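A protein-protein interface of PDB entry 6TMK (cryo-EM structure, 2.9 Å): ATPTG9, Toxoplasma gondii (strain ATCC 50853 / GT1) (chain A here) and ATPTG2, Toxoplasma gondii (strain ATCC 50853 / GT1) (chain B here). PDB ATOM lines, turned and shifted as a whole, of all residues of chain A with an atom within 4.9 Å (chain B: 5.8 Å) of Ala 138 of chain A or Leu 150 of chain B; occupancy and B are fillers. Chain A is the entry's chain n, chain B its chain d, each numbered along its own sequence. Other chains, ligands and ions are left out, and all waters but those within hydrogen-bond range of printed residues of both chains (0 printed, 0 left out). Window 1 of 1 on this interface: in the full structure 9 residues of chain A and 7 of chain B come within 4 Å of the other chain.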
ATOM      1  N   LEU A 134     -15.667   6.710   8.323  1.00  0.00           N
ATOM      2  CA  LEU A 134     -15.070   7.581   7.317  1.00  0.00           C
ATOM      3  C   LEU A 134     -16.141   8.267   6.476  1.00  0.00           C
ATOM      4  O   LEU A 134     -16.075   9.478   6.227  1.00  0.00           O
ATOM      5  CB  LEU A 134     -14.123   6.781   6.430  1.00  0.00           C
ATOM      6  CG  LEU A 134     -12.911   6.166   7.118  1.00  0.00           C
ATOM      7  CD1 LEU A 134     -12.236   5.181   6.204  1.00  0.00           C
ATOM      8  CD2 LEU A 134     -11.933   7.234   7.547  1.00  0.00           C
ATOM      9  N   ASP A 135     -17.136   7.502   6.023  1.00  0.00           N
ATOM     10  CA  ASP A 135     -18.251   8.081   5.279  1.00  0.00           C
ATOM     11  C   ASP A 135     -18.950   9.162   6.092  1.00  0.00           C
ATOM     12  O   ASP A 135     -19.272  10.237   5.574  1.00  0.00           O
ATOM     13  CB  ASP A 135     -19.233   6.983   4.885  1.00  0.00           C
ATOM     14  CG  ASP A 135     -18.676   6.057   3.823  1.00  0.00           C
ATOM     15  OD1 ASP A 135     -18.727   4.825   4.021  1.00  0.00           O
ATOM     16  OD2 ASP A 135     -18.177   6.557   2.795  1.00  0.00           O
ATOM     17  N   ARG A 136     -19.212   8.881   7.367  1.00  0.00           N
ATOM     18  CA  ARG A 136     -19.903   9.838   8.222  1.00  0.00           C
ATOM     19  C   ARG A 136     -19.121  11.139   8.314  1.00  0.00           C
ATOM     20  O   ARG A 136     -19.678  12.233   8.156  1.00  0.00           O
ATOM     21  CB  ARG A 136     -20.105   9.241   9.612  1.00  0.00           C
ATOM     22  CG  ARG A 136     -21.473   9.480  10.208  1.00  0.00           C
ATOM     23  CD  ARG A 136     -21.616   8.736  11.519  1.00  0.00           C
ATOM     24  NE  ARG A 136     -21.624   7.291  11.320  1.00  0.00           N
ATOM     25  CZ  ARG A 136     -21.286   6.402  12.250  1.00  0.00           C
ATOM     26  NH1 ARG A 136     -20.918   6.798  13.461  1.00  0.00           N
ATOM     27  NH2 ARG A 136     -21.320   5.109  11.965  1.00  0.00           N
ATOM     28  N   VAL A 137     -17.818  11.034   8.581  1.00  0.00           N
ATOM     29  CA  VAL A 137     -16.991  12.223   8.744  1.00  0.00           C
ATOM     30  C   VAL A 137     -16.946  13.018   7.447  1.00  0.00           C
ATOM     31  O   VAL A 137     -17.033  14.254   7.454  1.00  0.00           O
ATOM     32  CB  VAL A 137     -15.581  11.808   9.202  1.00  0.00           C
ATOM     33  CG1 VAL A 137     -14.643  12.992   9.216  1.00  0.00           C
ATOM     34  CG2 VAL A 137     -15.640  11.167  10.559  1.00  0.00           C
ATOM     35  N   ALA A 138     -16.813  12.328   6.316  1.00  0.00           N
ATOM     36  CA  ALA A 138     -16.745  13.028   5.041  1.00  0.00           C
ATOM     37  C   ALA A 138     -18.051  13.743   4.732  1.00  0.00           C
ATOM     38  O   ALA A 138     -18.045  14.881   4.248  1.00  0.00           O
ATOM     39  CB  ALA A 138     -16.398  12.043   3.930  1.00  0.00           C
ATOM     40  N   ASP A 139     -19.183  13.091   5.005  1.00  0.00           N
ATOM     41  CA  ASP A 139     -20.476  13.726   4.785  1.00  0.00           C
ATOM     42  C   ASP A 139     -20.645  14.950   5.671  1.00  0.00           C
ATOM     43  O   ASP A 139     -21.144  15.991   5.222  1.00  0.00           O
ATOM     44  CB  ASP A 139     -21.592  12.719   5.041  1.00  0.00           C
ATOM     45  CG  ASP A 139     -21.553  11.552   4.080  1.00  0.00           C
ATOM     46  OD1 ASP A 139     -22.391  10.638   4.216  1.00  0.00           O
ATOM     47  OD2 ASP A 139     -20.679  11.547   3.188  1.00  0.00           O
ATOM     48  N   SER A 140     -20.233  14.845   6.933  1.00  0.00           N
ATOM     49  CA  SER A 140     -20.328  15.983   7.835  1.00  0.00           C
ATOM     50  C   SER A 140     -19.487  17.150   7.338  1.00  0.00           C
ATOM     51  O   SER A 140     -19.934  18.304   7.357  1.00  0.00           O
ATOM     52  CB  SER A 140     -19.896  15.572   9.238  1.00  0.00           C
ATOM     53  N   LEU A 141     -18.260  16.872   6.896  1.00  0.00           N
ATOM     54  CA  LEU A 141     -17.408  17.940   6.390  1.00  0.00           C
ATOM     55  C   LEU A 141     -18.001  18.575   5.141  1.00  0.00           C
ATOM     56  O   LEU A 141     -17.967  19.801   4.985  1.00  0.00           O
ATOM     57  CB  LEU A 141     -16.010  17.407   6.104  1.00  0.00           C
ATOM     58  CG  LEU A 141     -15.221  16.923   7.315  1.00  0.00           C
ATOM     59  CD1 LEU A 141     -14.078  16.034   6.887  1.00  0.00           C
ATOM     60  CD2 LEU A 141     -14.705  18.096   8.104  1.00  0.00           C
ATOM     61  N   LYS A 142     -18.538  17.760   4.230  1.00  0.00           N
ATOM     62  CA  LYS A 142     -19.188  18.311   3.047  1.00  0.00           C
ATOM     63  C   LYS A 142     -20.340  19.226   3.428  1.00  0.00           C
ATOM     64  O   LYS A 142     -20.495  20.313   2.858  1.00  0.00           O
ATOM     65  CB  LYS A 142     -19.692  17.188   2.149  1.00  0.00           C
ATOM     66  CG  LYS A 142     -18.625  16.487   1.380  1.00  0.00           C
ATOM     67  CD  LYS A 142     -19.183  15.315   0.620  1.00  0.00           C
ATOM     68  CE  LYS A 142     -18.189  14.174   0.566  1.00  0.00           C
ATOM     69  NZ  LYS A 142     -18.711  13.015  -0.200  1.00  0.00           N
ATOM     70  N   LEU A 145     -18.993  22.510   4.867  1.00  0.00           N
ATOM     71  CA  LEU A 145     -18.369  23.360   3.859  1.00  0.00           C
ATOM     72  C   LEU A 145     -19.404  23.990   2.938  1.00  0.00           C
ATOM     73  O   LEU A 145     -19.372  25.200   2.690  1.00  0.00           O
ATOM     74  CB  LEU A 145     -17.366  22.547   3.050  1.00  0.00           C
ATOM     75  CG  LEU A 145     -16.102  22.125   3.785  1.00  0.00           C
ATOM     76  CD1 LEU A 145     -15.346  21.122   2.970  1.00  0.00           C
ATOM     77  CD2 LEU A 145     -15.239  23.326   4.065  1.00  0.00           C
ATOM     78  N   TYR A 150     -18.171  20.406  -5.709  1.00  0.00           N
ATOM     79  CA  TYR A 150     -17.571  19.149  -5.295  1.00  0.00           C
ATOM     80  C   TYR A 150     -18.150  17.998  -6.104  1.00  0.00           C
ATOM     81  O   TYR A 150     -19.368  17.894  -6.276  1.00  0.00           O
ATOM     82  CB  TYR A 150     -17.788  18.918  -3.803  1.00  0.00           C
ATOM     83  CG  TYR A 150     -16.887  17.850  -3.239  1.00  0.00           C
ATOM     84  CD1 TYR A 150     -15.582  18.141  -2.893  1.00  0.00           C
ATOM     85  CD2 TYR A 150     -17.338  16.556  -3.056  1.00  0.00           C
ATOM     86  CE1 TYR A 150     -14.749  17.178  -2.387  1.00  0.00           C
ATOM     87  CE2 TYR A 150     -16.512  15.583  -2.547  1.00  0.00           C
ATOM     88  CZ  TYR A 150     -15.217  15.898  -2.212  1.00  0.00           C
ATOM     89  OH  TYR A 150     -14.384  14.929  -1.703  1.00  0.00           O
ATOM     90  N   VAL B 145      -8.095   9.678   1.400  1.00  0.00           N
ATOM     91  CA  VAL B 145      -7.627  10.820   0.621  1.00  0.00           C
ATOM     92  C   VAL B 145      -8.715  11.881   0.506  1.00  0.00           C
ATOM     93  O   VAL B 145      -8.432  13.086   0.515  1.00  0.00           O
ATOM     94  CB  VAL B 145      -7.155  10.346  -0.764  1.00  0.00           C
ATOM     95  CG1 VAL B 145      -6.842  11.523  -1.650  1.00  0.00           C
ATOM     96  CG2 VAL B 145      -5.950   9.466  -0.628  1.00  0.00           C
ATOM     97  N   ASP B 146      -9.970  11.455   0.370  1.00  0.00           N
ATOM     98  CA  ASP B 146     -11.079  12.394   0.318  1.00  0.00           C
ATOM     99  C   ASP B 146     -11.166  13.199   1.601  1.00  0.00           C
ATOM    100  O   ASP B 146     -11.419  14.408   1.570  1.00  0.00           O
ATOM    101  CB  ASP B 146     -12.383  11.641   0.070  1.00  0.00           C
ATOM    102  CG  ASP B 146     -12.477  11.080  -1.333  1.00  0.00           C
ATOM    103  OD1 ASP B 146     -13.244  10.116  -1.540  1.00  0.00           O
ATOM    104  OD2 ASP B 146     -11.780  11.596  -2.232  1.00  0.00           O
ATOM    105  N   ILE B 147     -10.959  12.543   2.741  1.00  0.00           N
ATOM    106  CA  ILE B 147     -11.000  13.265   4.007  1.00  0.00           C
ATOM    107  C   ILE B 147      -9.888  14.302   4.057  1.00  0.00           C
ATOM    108  O   ILE B 147     -10.097  15.443   4.491  1.00  0.00           O
ATOM    109  CB  ILE B 147     -10.919  12.289   5.191  1.00  0.00           C
ATOM    110  CG1 ILE B 147     -12.202  11.468   5.275  1.00  0.00           C
ATOM    111  CG2 ILE B 147     -10.686  13.039   6.478  1.00  0.00           C
ATOM    112  CD1 ILE B 147     -12.081  10.253   6.116  1.00  0.00           C
ATOM    113  N   THR B 148      -8.686  13.925   3.620  1.00  0.00           N
ATOM    114  CA  THR B 148      -7.586  14.887   3.645  1.00  0.00           C
ATOM    115  C   THR B 148      -7.865  16.072   2.725  1.00  0.00           C
ATOM    116  O   THR B 148      -7.564  17.223   3.069  1.00  0.00           O
ATOM    117  CB  THR B 148      -6.272  14.207   3.272  1.00  0.00           C
ATOM    118  OG1 THR B 148      -6.359  13.654   1.955  1.00  0.00           O
ATOM    119  CG2 THR B 148      -5.943  13.124   4.267  1.00  0.00           C
ATOM    120  N   SER B 149      -8.446  15.815   1.552  1.00  0.00           N
ATOM    121  CA  SER B 149      -8.793  16.906   0.647  1.00  0.00           C
ATOM    122  C   SER B 149      -9.853  17.813   1.255  1.00  0.00           C
ATOM    123  O   SER B 149      -9.806  19.038   1.090  1.00  0.00           O
ATOM    124  CB  SER B 149      -9.273  16.350  -0.688  1.00  0.00           C
ATOM    125  OG  SER B 149      -8.328  15.453  -1.231  1.00  0.00           O
ATOM    126  N   LEU B 150     -10.830  17.231   1.946  1.00  0.00           N
ATOM    127  CA  LEU B 150     -11.861  18.040   2.578  1.00  0.00           C
ATOM    128  C   LEU B 150     -11.273  18.905   3.682  1.00  0.00           C
ATOM    129  O   LEU B 150     -11.709  20.041   3.890  1.00  0.00           O
ATOM    130  CB  LEU B 150     -12.961  17.141   3.125  1.00  0.00           C
ATOM    131  CG  LEU B 150     -13.814  16.458   2.067  1.00  0.00           C
ATOM    132  CD1 LEU B 150     -14.566  15.299   2.667  1.00  0.00           C
ATOM    133  CD2 LEU B 150     -14.769  17.436   1.449  1.00  0.00           C
ATOM    134  N   LEU B 151     -10.278  18.388   4.398  1.00  0.00           N
ATOM    135  CA  LEU B 151      -9.641  19.205   5.423  1.00  0.00           C
ATOM    136  C   LEU B 151      -8.798  20.313   4.811  1.00  0.00           C
ATOM    137  O   LEU B 151      -8.711  21.410   5.373  1.00  0.00           O
ATOM    138  CB  LEU B 151      -8.797  18.327   6.335  1.00  0.00           C
ATOM    139  CG  LEU B 151      -9.600  17.315   7.139  1.00  0.00           C
ATOM    140  CD1 LEU B 151      -8.675  16.401   7.853  1.00  0.00           C
ATOM    141  CD2 LEU B 151     -10.505  18.009   8.118  1.00  0.00           C
ATOM    142  N   GLU B 152      -8.190  20.057   3.655  1.00  0.00           N
ATOM    143  CA  GLU B 152      -7.522  21.132   2.931  1.00  0.00           C
ATOM    144  C   GLU B 152      -8.513  22.216   2.524  1.00  0.00           C
ATOM    145  O   GLU B 152      -8.224  23.413   2.643  1.00  0.00           O
ATOM    146  CB  GLU B 152      -6.794  20.571   1.715  1.00  0.00           C
ATOM    147  CG  GLU B 152      -5.539  19.808   2.065  1.00  0.00           C
ATOM    148  CD  GLU B 152      -5.183  18.751   1.039  1.00  0.00           C
ATOM    149  OE1 GLU B 152      -5.513  18.937  -0.149  1.00  0.00           O
ATOM    150  OE2 GLU B 152      -4.570  17.731   1.423  1.00  0.00           O
ATOM    151  N   LEU B 153      -9.681  21.815   2.024  1.00  0.00           N
ATOM    152  CA  LEU B 153     -10.716  22.786   1.686  1.00  0.00           C
ATOM    153  C   LEU B 153     -11.168  23.567   2.913  1.00  0.00           C
ATOM    154  O   LEU B 153     -11.439  24.769   2.827  1.00  0.00           O
ATOM    155  CB  LEU B 153     -11.908  22.084   1.044  1.00  0.00           C
ATOM    156  CG  LEU B 153     -11.673  21.547  -0.359  1.00  0.00           C
ATOM    157  CD1 LEU B 153     -12.755  20.570  -0.766  1.00  0.00           C
ATOM    158  CD2 LEU B 153     -11.613  22.694  -1.325  1.00  0.00           C
ATOM    159  N   GLN B 154     -11.275  22.898   4.056  1.00  0.00           N
ATOM    160  CA  GLN B 154     -11.666  23.582   5.281  1.00  0.00           C
ATOM    161  C   GLN B 154     -10.615  24.608   5.687  1.00  0.00           C
ATOM    162  O   GLN B 154     -10.947  25.710   6.140  1.00  0.00           O
ATOM    163  CB  GLN B 154     -11.881  22.548   6.380  1.00  0.00           C
ATOM    164  CG  GLN B 154     -12.645  23.023   7.575  1.00  0.00           C
ATOM    165  CD  GLN B 154     -12.908  21.906   8.556  1.00  0.00           C
ATOM    166  OE1 GLN B 154     -12.884  20.733   8.193  1.00  0.00           O
ATOM    167  NE2 GLN B 154     -13.155  22.262   9.808  1.00  0.00           N
ATOM    168  N   ALA B 155      -9.340  24.260   5.520  1.00  0.00           N
ATOM    169  CA  ALA B 155      -8.264  25.212   5.769  1.00  0.00           C
ATOM    170  C   ALA B 155      -8.378  26.421   4.853  1.00  0.00           C
ATOM    171  O   ALA B 155      -8.226  27.567   5.291  1.00  0.00           O
ATOM    172  CB  ALA B 155      -6.915  24.531   5.576  1.00  0.00           C
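Ile 147 of chain B touches Leu 134 of chain A.
Ala 138 of chain A touches Leu 150 of chain B (O to CD1, 3.8 Å).
OE1 of Gln 154 of chain B touches CD2 of Leu 141 of chain A, at 3.2 Å.
Lys 142 of chain A touches Leu 150 of chain B (CG to CD2, 3.97 Å).
Leu 145 of chain A touches Leu 150 of chain B (CD1 to O, 3.9 Å).
Gln 154 of chain B touches Leu 145 of chain A (CA to CD2, 3.8 Å).
Tyr 150 of chain A touches Leu 150 of chain B (CE1 to CD2, 3.8 Å).
Leu 150 of chain B touches four residues of chain A.
Printed residues of chain B within 4 Å of Leu 141 of chain A: Gln 154.
Of the printed residues of chain A, Ile 147 of chain B touches Leu 134.
Of the printed residues of chain B, Leu 134 of chain A touches Ile 147.
Ser 140 of chain A touches none of the printed residues of chain B.
The nearest residue of chain B that does not touch Ala 138 of chain A is Ile 147 of chain B (4.4 Å).
The nearest residue of chain A that does not touch Leu 150 of chain B is Leu 141 of chain A (4.1 Å).
The nearest printed residue of chain B that does not touch Leu 145 of chain A is Leu 153 of chain B (4.1 Å).
Hydrophobic or aromatic side chains of chain A within 4 Å of the printed part of chain B: Leu 134, Ala 138, Leu 141, Leu 145 and Tyr 150.
Along chain B the printed residues that touch a printed residue of chain A span positions 147 to 154.
Among the printed residues, 7 pairs touch across the chains.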
